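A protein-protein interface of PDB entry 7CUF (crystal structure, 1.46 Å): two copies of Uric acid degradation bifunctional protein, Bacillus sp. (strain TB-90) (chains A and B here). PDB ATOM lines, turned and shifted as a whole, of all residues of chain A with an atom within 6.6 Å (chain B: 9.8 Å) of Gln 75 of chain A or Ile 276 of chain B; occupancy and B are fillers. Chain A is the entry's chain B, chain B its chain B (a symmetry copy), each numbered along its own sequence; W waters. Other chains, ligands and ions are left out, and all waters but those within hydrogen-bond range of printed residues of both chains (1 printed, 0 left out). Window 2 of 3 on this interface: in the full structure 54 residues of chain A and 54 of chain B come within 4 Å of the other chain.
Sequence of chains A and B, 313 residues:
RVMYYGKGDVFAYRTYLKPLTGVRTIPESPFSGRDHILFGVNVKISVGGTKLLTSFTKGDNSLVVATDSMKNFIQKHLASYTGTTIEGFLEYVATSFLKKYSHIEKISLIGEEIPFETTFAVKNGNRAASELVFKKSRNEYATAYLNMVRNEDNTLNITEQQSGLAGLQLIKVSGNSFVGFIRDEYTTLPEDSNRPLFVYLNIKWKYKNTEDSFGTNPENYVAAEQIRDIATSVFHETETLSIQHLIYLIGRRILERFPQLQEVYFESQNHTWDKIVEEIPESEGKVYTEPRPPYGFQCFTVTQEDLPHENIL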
ATOM      1  N   ASP A   9      15.521  18.713  15.286  1.00  0.00           N
ATOM      2  CA  ASP A   9      15.241  19.824  16.190  1.00  0.00           C
ATOM      3  C   ASP A   9      13.914  19.653  16.921  1.00  0.00           C
ATOM      4  O   ASP A   9      13.161  20.599  17.090  1.00  0.00           O
ATOM      5  CB  ASP A   9      15.323  21.173  15.473  1.00  0.00           C
ATOM      6  CG  ASP A   9      16.755  21.650  15.289  1.00  0.00           C
ATOM      7  OD1 ASP A   9      17.689  21.051  15.869  1.00  0.00           O
ATOM      8  OD2 ASP A   9      16.926  22.641  14.561  1.00  0.00           O
ATOM      9  N   VAL A  10      13.637  18.433  17.384  1.00  0.00           N
ATOM     10  CA  VAL A  10      12.502  18.192  18.279  1.00  0.00           C
ATOM     11  C   VAL A  10      12.939  18.543  19.692  1.00  0.00           C
ATOM     12  O   VAL A  10      13.464  17.688  20.424  1.00  0.00           O
ATOM     13  CB  VAL A  10      11.986  16.749  18.196  1.00  0.00           C
ATOM     14  CG1 VAL A  10      10.741  16.609  19.070  1.00  0.00           C
ATOM     15  CG2 VAL A  10      11.639  16.357  16.730  1.00  0.00           C
ATOM     16  N   PHE A  11      12.740  19.805  20.075  1.00  0.00           N
ATOM     17  CA  PHE A  11      13.043  20.256  21.424  1.00  0.00           C
ATOM     18  C   PHE A  11      11.940  19.819  22.367  1.00  0.00           C
ATOM     19  O   PHE A  11      10.746  19.848  22.026  1.00  0.00           O
ATOM     20  CB  PHE A  11      13.182  21.776  21.493  1.00  0.00           C
ATOM     21  CG  PHE A  11      14.382  22.284  20.799  1.00  0.00           C
ATOM     22  CD1 PHE A  11      14.346  22.505  19.433  1.00  0.00           C
ATOM     23  CD2 PHE A  11      15.550  22.517  21.495  1.00  0.00           C
ATOM     24  CE1 PHE A  11      15.452  22.951  18.771  1.00  0.00           C
ATOM     25  CE2 PHE A  11      16.656  22.961  20.842  1.00  0.00           C
ATOM     26  CZ  PHE A  11      16.611  23.178  19.474  1.00  0.00           C
ATOM     27  N   ALA A  12      12.336  19.374  23.544  1.00  0.00           N
ATOM     28  CA  ALA A  12      11.375  18.964  24.542  1.00  0.00           C
ATOM     29  C   ALA A  12      11.979  19.219  25.915  1.00  0.00           C
ATOM     30  O   ALA A  12      13.126  18.824  26.173  1.00  0.00           O
ATOM     31  CB  ALA A  12      10.974  17.492  24.355  1.00  0.00           C
ATOM     32  N   MET A  70       5.814  12.208  14.330  1.00  0.00           N
ATOM     33  CA  MET A  70       7.032  11.824  15.033  1.00  0.00           C
ATOM     34  C   MET A  70       7.375  12.799  16.149  1.00  0.00           C
ATOM     35  O   MET A  70       7.781  12.393  17.240  1.00  0.00           O
ATOM     36  CB  MET A  70       8.173  11.758  14.027  1.00  0.00           C
ATOM     37  CG  MET A  70       7.974  10.718  12.994  1.00  0.00           C
ATOM     38  SD  MET A  70       9.374  10.569  11.884  1.00  0.00           S
ATOM     39  CE  MET A  70       8.596   9.846  10.487  1.00  0.00           C
ATOM     40  N   LYS A  71       7.275  14.093  15.878  1.00  0.00           N
ATOM     41  CA  LYS A  71       7.474  15.130  16.900  1.00  0.00           C
ATOM     42  C   LYS A  71       6.487  14.929  18.049  1.00  0.00           C
ATOM     43  O   LYS A  71       6.872  14.923  19.222  1.00  0.00           O
ATOM     44  CB  LYS A  71       7.299  16.510  16.272  1.00  0.00           C
ATOM     45  CG  LYS A  71       7.375  17.731  17.181  1.00  0.00           C
ATOM     46  CD  LYS A  71       5.989  18.307  17.491  1.00  0.00           C
ATOM     47  CE  LYS A  71       5.192  18.761  16.293  1.00  0.00           C
ATOM     48  N   ASN A  72       5.199  14.746  17.730  1.00  0.00           N
ATOM     49  CA  ASN A  72       4.229  14.502  18.783  1.00  0.00           C
ATOM     50  C   ASN A  72       4.598  13.274  19.602  1.00  0.00           C
ATOM     51  O   ASN A  72       4.485  13.282  20.833  1.00  0.00           O
ATOM     52  CB  ASN A  72       2.836  14.310  18.168  1.00  0.00           C
ATOM     53  CG  ASN A  72       2.290  15.595  17.512  1.00  0.00           C
ATOM     54  OD1 ASN A  72       2.680  16.707  17.885  1.00  0.00           O
ATOM     55  ND2 ASN A  72       1.351  15.438  16.565  1.00  0.00           N
ATOM     56  N   PHE A  73       4.993  12.192  18.927  1.00  0.00           N
ATOM     57  CA  PHE A  73       5.373  10.955  19.582  1.00  0.00           C
ATOM     58  C   PHE A  73       6.471  11.199  20.597  1.00  0.00           C
ATOM     59  O   PHE A  73       6.363  10.788  21.758  1.00  0.00           O
ATOM     60  CB  PHE A  73       5.847   9.969  18.526  1.00  0.00           C
ATOM     61  CG  PHE A  73       5.943   8.558  18.998  1.00  0.00           C
ATOM     62  CD1 PHE A  73       7.120   8.088  19.601  1.00  0.00           C
ATOM     63  CD2 PHE A  73       4.891   7.673  18.819  1.00  0.00           C
ATOM     64  CE1 PHE A  73       7.212   6.770  20.009  1.00  0.00           C
ATOM     65  CE2 PHE A  73       4.985   6.377  19.218  1.00  0.00           C
ATOM     66  CZ  PHE A  73       6.159   5.923  19.824  1.00  0.00           C
ATOM     67  N   ILE A  74       7.539  11.878  20.173  1.00  0.00           N
ATOM     68  CA  ILE A  74       8.670  12.124  21.063  1.00  0.00           C
ATOM     69  C   ILE A  74       8.242  12.940  22.273  1.00  0.00           C
ATOM     70  O   ILE A  74       8.599  12.624  23.418  1.00  0.00           O
ATOM     71  CB  ILE A  74       9.809  12.842  20.314  1.00  0.00           C
ATOM     72  CG1 ILE A  74      10.417  11.922  19.241  1.00  0.00           C
ATOM     73  CG2 ILE A  74      10.868  13.329  21.307  1.00  0.00           C
ATOM     74  CD1 ILE A  74      11.253  12.622  18.209  1.00  0.00           C
ATOM     75  N   GLN A  75       7.524  14.044  22.036  1.00  0.00           N
ATOM     76  CA  GLN A  75       7.117  14.921  23.125  1.00  0.00           C
ATOM     77  C   GLN A  75       6.223  14.188  24.106  1.00  0.00           C
ATOM     78  O   GLN A  75       6.390  14.311  25.326  1.00  0.00           O
ATOM     79  CB  GLN A  75       6.501  16.198  22.534  1.00  0.00           C
ATOM     80  CG  GLN A  75       7.513  16.882  21.615  1.00  0.00           C
ATOM     81  CD  GLN A  75       7.033  18.192  21.016  1.00  0.00           C
ATOM     82  OE1 GLN A  75       5.858  18.341  20.688  1.00  0.00           O
ATOM     83  NE2 GLN A  75       7.978  19.131  20.802  1.00  0.00           N
ATOM     84  N   LYS A  76       5.297  13.377  23.598  1.00  0.00           N
ATOM     85  CA  LYS A  76       4.406  12.654  24.501  1.00  0.00           C
ATOM     86  C   LYS A  76       5.179  11.626  25.306  1.00  0.00           C
ATOM     87  O   LYS A  76       4.909  11.423  26.486  1.00  0.00           O
ATOM     88  CB  LYS A  76       3.282  11.986  23.711  1.00  0.00           C
ATOM     89  CG  LYS A  76       2.288  13.003  23.185  1.00  0.00           C
ATOM     90  CD  LYS A  76       1.232  12.371  22.268  1.00  0.00           C
ATOM     91  CE  LYS A  76      -0.123  13.047  22.419  1.00  0.00           C
ATOM     92  NZ  LYS A  76      -1.174  12.233  21.770  1.00  0.00           N
ATOM     93  N   HIS A  77       6.167  10.981  24.686  1.00  0.00           N
ATOM     94  CA  HIS A  77       6.959   9.999  25.408  1.00  0.00           C
ATOM     95  C   HIS A  77       7.886  10.620  26.433  1.00  0.00           C
ATOM     96  O   HIS A  77       8.213   9.963  27.429  1.00  0.00           O
ATOM     97  CB  HIS A  77       7.673   9.112  24.402  1.00  0.00           C
ATOM     98  CG  HIS A  77       6.814   8.028  23.859  1.00  0.00           C
ATOM     99  ND1 HIS A  77       5.810   8.280  22.948  1.00  0.00           N
ATOM    100  CD2 HIS A  77       6.721   6.715  24.165  1.00  0.00           C
ATOM    101  CE1 HIS A  77       5.180   7.154  22.667  1.00  0.00           C
ATOM    102  NE2 HIS A  77       5.711   6.192  23.400  1.00  0.00           N
ATOM    103  N   LEU A  78       8.273  11.877  26.275  1.00  0.00           N
ATOM    104  CA  LEU A  78       9.032  12.505  27.348  1.00  0.00           C
ATOM    105  C   LEU A  78       8.152  12.681  28.571  1.00  0.00           C
ATOM    106  O   LEU A  78       8.639  12.593  29.706  1.00  0.00           O
ATOM    107  CB  LEU A  78       9.650  13.839  26.896  1.00  0.00           C
ATOM    108  CG  LEU A  78      10.608  14.467  27.915  1.00  0.00           C
ATOM    109  CD1 LEU A  78      11.739  13.569  28.267  1.00  0.00           C
ATOM    110  CD2 LEU A  78      11.181  15.785  27.412  1.00  0.00           C
ATOM    111  N   ALA A  79       6.872  12.945  28.368  1.00  0.00           N
ATOM    112  CA  ALA A  79       5.950  13.088  29.488  1.00  0.00           C
ATOM    113  C   ALA A  79       5.732  11.763  30.223  1.00  0.00           C
ATOM    114  O   ALA A  79       5.559  11.773  31.443  1.00  0.00           O
ATOM    115  CB  ALA A  79       4.586  13.618  28.996  1.00  0.00           C
ATOM    116  N   SER A  80       5.759  10.631  29.534  1.00  0.00           N
ATOM    117  CA  SER A  80       5.552   9.368  30.229  1.00  0.00           C
ATOM    118  C   SER A  80       6.842   8.682  30.660  1.00  0.00           C
ATOM    119  O   SER A  80       6.782   7.694  31.399  1.00  0.00           O
ATOM    120  CB  SER A  80       4.731   8.416  29.365  1.00  0.00           C
ATOM    121  OG  SER A  80       5.278   8.286  28.089  1.00  0.00           O
ATOM    122  N   PHE A  89      15.984   7.426  27.667  1.00  0.00           N
ATOM    123  CA  PHE A  89      14.867   8.026  26.962  1.00  0.00           C
ATOM    124  C   PHE A  89      14.874   7.592  25.515  1.00  0.00           C
ATOM    125  O   PHE A  89      13.840   7.212  24.971  1.00  0.00           O
ATOM    126  CB  PHE A  89      14.917   9.568  27.073  1.00  0.00           C
ATOM    127  CG  PHE A  89      13.799  10.248  26.315  1.00  0.00           C
ATOM    128  CD1 PHE A  89      12.467   9.927  26.565  1.00  0.00           C
ATOM    129  CD2 PHE A  89      14.067  11.179  25.340  1.00  0.00           C
ATOM    130  CE1 PHE A  89      11.444  10.542  25.849  1.00  0.00           C
ATOM    131  CE2 PHE A  89      13.035  11.762  24.627  1.00  0.00           C
ATOM    132  CZ  PHE A  89      11.733  11.421  24.873  1.00  0.00           C
ATOM    133  N   PRO B 196       6.174  28.993  32.794  1.00  0.00           N
ATOM    134  CA  PRO B 196       7.628  28.889  33.037  1.00  0.00           C
ATOM    135  C   PRO B 196       8.392  30.002  32.333  1.00  0.00           C
ATOM    136  O   PRO B 196       9.079  29.805  31.309  1.00  0.00           O
ATOM    137  CB  PRO B 196       7.939  27.510  32.460  1.00  0.00           C
ATOM    138  CG  PRO B 196       7.021  27.402  31.282  1.00  0.00           C
ATOM    139  CD  PRO B 196       5.754  28.161  31.649  1.00  0.00           C
ATOM    140  N   TRP B 273       8.649  28.927  26.671  1.00  0.00           N
ATOM    141  CA  TRP B 273       8.283  27.807  25.847  1.00  0.00           C
ATOM    142  C   TRP B 273       6.770  27.594  25.814  1.00  0.00           C
ATOM    143  O   TRP B 273       6.024  27.991  26.722  1.00  0.00           O
ATOM    144  CB  TRP B 273       8.890  26.520  26.426  1.00  0.00           C
ATOM    145  CG  TRP B 273      10.378  26.588  26.635  1.00  0.00           C
ATOM    146  CD1 TRP B 273      11.290  27.126  25.794  1.00  0.00           C
ATOM    147  CD2 TRP B 273      11.100  26.071  27.750  1.00  0.00           C
ATOM    148  NE1 TRP B 273      12.543  27.025  26.329  1.00  0.00           N
ATOM    149  CE2 TRP B 273      12.462  26.334  27.514  1.00  0.00           C
ATOM    150  CE3 TRP B 273      10.737  25.417  28.929  1.00  0.00           C
ATOM    151  CZ2 TRP B 273      13.454  25.992  28.422  1.00  0.00           C
ATOM    152  CZ3 TRP B 273      11.727  25.062  29.813  1.00  0.00           C
ATOM    153  CH2 TRP B 273      13.080  25.342  29.537  1.00  0.00           C
ATOM    154  N   ASP B 274       6.332  26.911  24.754  1.00  0.00           N
ATOM    155  CA  ASP B 274       4.941  26.528  24.604  1.00  0.00           C
ATOM    156  C   ASP B 274       4.683  25.193  25.287  1.00  0.00           C
ATOM    157  O   ASP B 274       5.463  24.249  25.160  1.00  0.00           O
ATOM    158  CB  ASP B 274       4.616  26.338  23.111  1.00  0.00           C
ATOM    159  CG  ASP B 274       4.460  27.646  22.337  1.00  0.00           C
ATOM    160  OD1 ASP B 274       4.175  28.710  22.933  1.00  0.00           O
ATOM    161  OD2 ASP B 274       4.629  27.582  21.091  1.00  0.00           O
ATOM    162  N   LYS B 275       3.533  25.086  25.927  1.00  0.00           N
ATOM    163  CA  LYS B 275       3.164  23.879  26.648  1.00  0.00           C
ATOM    164  C   LYS B 275       2.594  22.821  25.702  1.00  0.00           C
ATOM    165  O   LYS B 275       1.822  23.118  24.783  1.00  0.00           O
ATOM    166  CB  LYS B 275       2.169  24.218  27.769  1.00  0.00           C
ATOM    167  CG  LYS B 275       1.797  23.058  28.690  1.00  0.00           C
ATOM    168  N   ILE B 276       2.999  21.585  25.943  1.00  0.00           N
ATOM    169  CA  ILE B 276       2.598  20.419  25.171  1.00  0.00           C
ATOM    170  C   ILE B 276       1.772  19.461  26.020  1.00  0.00           C
ATOM    171  O   ILE B 276       0.706  19.000  25.596  1.00  0.00           O
ATOM    172  CB  ILE B 276       3.833  19.690  24.584  1.00  0.00           C
ATOM    173  CG1 ILE B 276       4.574  20.571  23.571  1.00  0.00           C
ATOM    174  CG2 ILE B 276       3.426  18.368  23.945  1.00  0.00           C
ATOM    175  CD1 ILE B 276       3.630  21.240  22.544  1.00  0.00           C
ATOM    176  N   VAL B 277       2.254  19.142  27.225  1.00  0.00           N
ATOM    177  CA  VAL B 277       1.618  18.177  28.118  1.00  0.00           C
ATOM    178  C   VAL B 277       1.437  18.835  29.478  1.00  0.00           C
ATOM    179  O   VAL B 277       2.420  19.259  30.100  1.00  0.00           O
ATOM    180  CB  VAL B 277       2.436  16.879  28.246  1.00  0.00           C
ATOM    181  N   GLU B 278       0.176  18.901  29.939  1.00  0.00           N
ATOM    182  CA  GLU B 278      -0.183  19.585  31.174  1.00  0.00           C
ATOM    183  C   GLU B 278      -0.239  18.641  32.372  1.00  0.00           C
ATOM    184  O   GLU B 278       0.240  18.997  33.455  1.00  0.00           O
ATOM    185  CB  GLU B 278      -1.553  20.260  31.024  1.00  0.00           C
ATOM    186  N   GLU B 279      -0.819  17.449  32.206  1.00  0.00           N
ATOM    187  CA  GLU B 279      -1.073  16.531  33.314  1.00  0.00           C
ATOM    188  C   GLU B 279      -0.321  15.225  33.086  1.00  0.00           C
ATOM    189  O   GLU B 279      -0.699  14.427  32.222  1.00  0.00           O
ATOM    190  CB  GLU B 279      -2.575  16.265  33.458  1.00  0.00           C
ATOM    191  N   ILE B 280       0.722  14.996  33.872  1.00  0.00           N
ATOM    192  CA  ILE B 280       1.472  13.740  33.857  1.00  0.00           C
ATOM    193  C   ILE B 280       1.031  12.902  35.054  1.00  0.00           C
ATOM    194  O   ILE B 280       1.027  13.416  36.184  1.00  0.00           O
ATOM    195  CB  ILE B 280       2.991  13.990  33.898  1.00  0.00           C
ATOM    196  CG1 ILE B 280       3.407  14.904  32.743  1.00  0.00           C
ATOM    197  CG2 ILE B 280       3.740  12.668  33.826  1.00  0.00           C
ATOM    198  CD1 ILE B 280       4.872  15.323  32.762  1.00  0.00           C
ATOM    199  N   GLY B 285       5.378  17.101  36.945  1.00  0.00           N
ATOM    200  CA  GLY B 285       6.047  17.549  35.742  1.00  0.00           C
ATOM    201  C   GLY B 285       5.084  17.851  34.596  1.00  0.00           C
ATOM    202  O   GLY B 285       3.908  17.483  34.598  1.00  0.00           O
ATOM    203  N   LYS B 286       5.637  18.511  33.584  1.00  0.00           N
ATOM    204  CA  LYS B 286       4.930  18.904  32.378  1.00  0.00           C
ATOM    205  C   LYS B 286       5.959  18.808  31.255  1.00  0.00           C
ATOM    206  O   LYS B 286       7.167  18.667  31.525  1.00  0.00           O
ATOM    207  CB  LYS B 286       4.436  20.336  32.530  1.00  0.00           C
ATOM    208  CG  LYS B 286       3.441  20.550  33.697  1.00  0.00           C
ATOM    209  CD  LYS B 286       2.804  21.926  33.590  1.00  0.00           C
ATOM    210  N   VAL B 287       5.510  18.895  30.000  1.00  0.00           N
ATOM    211  CA  VAL B 287       6.438  18.994  28.851  1.00  0.00           C
ATOM    212  C   VAL B 287       6.158  20.246  28.034  1.00  0.00           C
ATOM    213  O   VAL B 287       5.000  20.555  27.731  1.00  0.00           O
ATOM    214  CB  VAL B 287       6.414  17.746  27.954  1.00  0.00           C
ATOM    215  CG1 VAL B 287       7.310  17.932  26.712  1.00  0.00           C
ATOM    216  CG2 VAL B 287       6.831  16.513  28.716  1.00  0.00           C
ATOM    217  N   TYR B 288       7.230  20.951  27.661  1.00  0.00           N
ATOM    218  CA  TYR B 288       7.154  22.165  26.874  1.00  0.00           C
ATOM    219  C   TYR B 288       8.071  22.062  25.664  1.00  0.00           C
ATOM    220  O   TYR B 288       8.915  21.183  25.601  1.00  0.00           O
ATOM    221  CB  TYR B 288       7.615  23.361  27.692  1.00  0.00           C
ATOM    222  CG  TYR B 288       6.920  23.503  28.993  1.00  0.00           C
ATOM    223  CD1 TYR B 288       7.323  22.810  30.115  1.00  0.00           C
ATOM    224  CD2 TYR B 288       5.854  24.375  29.104  1.00  0.00           C
ATOM    225  CE1 TYR B 288       6.697  22.976  31.324  1.00  0.00           C
ATOM    226  CE2 TYR B 288       5.177  24.532  30.306  1.00  0.00           C
ATOM    227  CZ  TYR B 288       5.610  23.840  31.407  1.00  0.00           C
ATOM    228  OH  TYR B 288       4.972  23.994  32.602  1.00  0.00           O
ATOM    229  N   THR B 289       7.869  22.931  24.679  1.00  0.00           N
ATOM    230  CA  THR B 289       8.704  22.947  23.486  1.00  0.00           C
ATOM    231  C   THR B 289       9.000  24.388  23.054  1.00  0.00           C
ATOM    232  O   THR B 289       8.439  25.350  23.568  1.00  0.00           O
ATOM    233  CB  THR B 289       8.094  22.091  22.354  1.00  0.00           C
ATOM    234  OG1 THR B 289       9.131  21.844  21.376  1.00  0.00           O
ATOM    235  CG2 THR B 289       6.866  22.761  21.752  1.00  0.00           C
ATOM    236  N   GLU B 290       9.934  24.533  22.110  1.00  0.00           N
ATOM    237  CA  GLU B 290      10.326  25.862  21.633  1.00  0.00           C
ATOM    238  C   GLU B 290       9.175  26.545  20.894  1.00  0.00           C
ATOM    239  O   GLU B 290       8.443  25.883  20.152  1.00  0.00           O
ATOM    240  CB  GLU B 290      11.525  25.757  20.677  1.00  0.00           C
ATOM    241  CG  GLU B 290      12.861  25.398  21.289  1.00  0.00           C
ATOM    242  CD  GLU B 290      13.360  26.451  22.244  1.00  0.00           C
ATOM    243  OE1 GLU B 290      14.184  26.135  23.094  1.00  0.00           O
ATOM    244  OE2 GLU B 290      12.877  27.599  22.175  1.00  0.00           O
ATOM    245  N   PRO B 291       9.015  27.862  21.052  1.00  0.00           N
ATOM    246  CA  PRO B 291       7.904  28.585  20.417  1.00  0.00           C
ATOM    247  C   PRO B 291       8.283  28.923  18.975  1.00  0.00           C
ATOM    248  O   PRO B 291       9.379  28.619  18.505  1.00  0.00           O
ATOM    249  CB  PRO B 291       7.825  29.860  21.278  1.00  0.00           C
ATOM    250  CG  PRO B 291       9.220  30.089  21.735  1.00  0.00           C
ATOM    251  CD  PRO B 291       9.811  28.737  21.943  1.00  0.00           C
HETATM  252  O   HOH W   1      11.456  22.094  18.829  1.00  0.00           O
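Of the printed residues of chain B, Gln 75 of chain A touches Ile 276 (3.9 Å), Val 287 (3.98 Å) and Thr 289 (3.0 Å).
Of chain A, only Gln 75 (3.9 Å) comes within 4 Å of Ile 276 of chain B.
Ile 74 of chain A touches none of the printed residues of chain B.
Printed residues of chain B within 4 Å of Ala 12 of chain A: Tyr 288.
Of the printed residues of chain A, Ile 280 of chain B touches Ala 79.
Printed residues of chain B within 4 Å of Phe 11 of chain A: Thr 289 (2.6 Å) and Glu 290 (3.5 Å).
The nearest residue of chain A that does not touch Ile 276 of chain B is Lys 76 of chain A (5.3 Å).
Water W1 lies within hydrogen-bond range of the backbone carbonyl oxygen of Asp 9 of chain A, the backbone NH of Phe 11 of chain A and the side-chain hydroxyl of Thr 289 of chain B.
O of Phe 11 of chain A lies within hydrogen-bond range of NE2 of Gln 75 of chain A.
The backbone carbonyl oxygen (O) of Asp 274 of chain B sits at hydrogen-bond distance from the backbone NH (N) of Thr 289 of chain B, at 2.8 Å.
The backbone carbonyl oxygen (O) of Val 287 of chain B is in hydrogen-bond range of the backbone NH (N) of Ile 276 of chain B (2.9 Å).
The backbone carbonyl oxygen of Val 277 of chain B sits at hydrogen-bond distance from the backbone NH of Val 287 of chain B, at 3.1 Å.
Hydrophobic or aromatic side chains of chain A that line the printed part of chain B: Phe 11 and Ala 79.
Of the 16 printed residues of chain B, 7 touch a printed residue of chain A.
Hydrophobic or aromatic side chains of chain B that line the printed part of chain A: Ile 276, Val 277, Ile 280 and Val 287.
Among the printed residues, 9 pairs touch across the chains.
No position is printed for both chains.
The backbone carbonyl oxygen (O) of Phe 11 of chain A sits at hydrogen-bond distance from the side-chain hydroxyl (OG1) of Thr 289 of chain B, 2.6 Å away.
The side-chain amide nitrogen (NE2) of Gln 75 of chain A lies within hydrogen-bond range of the side-chain hydroxyl (OG1) of Thr 289 of chain B (3.0 Å).
Among the printed residues, pairs that only touch across the chains: Phe 11 of chain A with Glu 290 of chain B, Ala 12 of chain A with Tyr 288 of chain B, Gln 75 of chain A with Ile 276 of chain B, Gln 75 of chain A with Val 287 of chain B, Ala 79 of chain A with Val 277 of chain B, Ala 79 of chain A with Ile 280 of chain B and Ala 79 of chain A with Val 287 of chain B.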
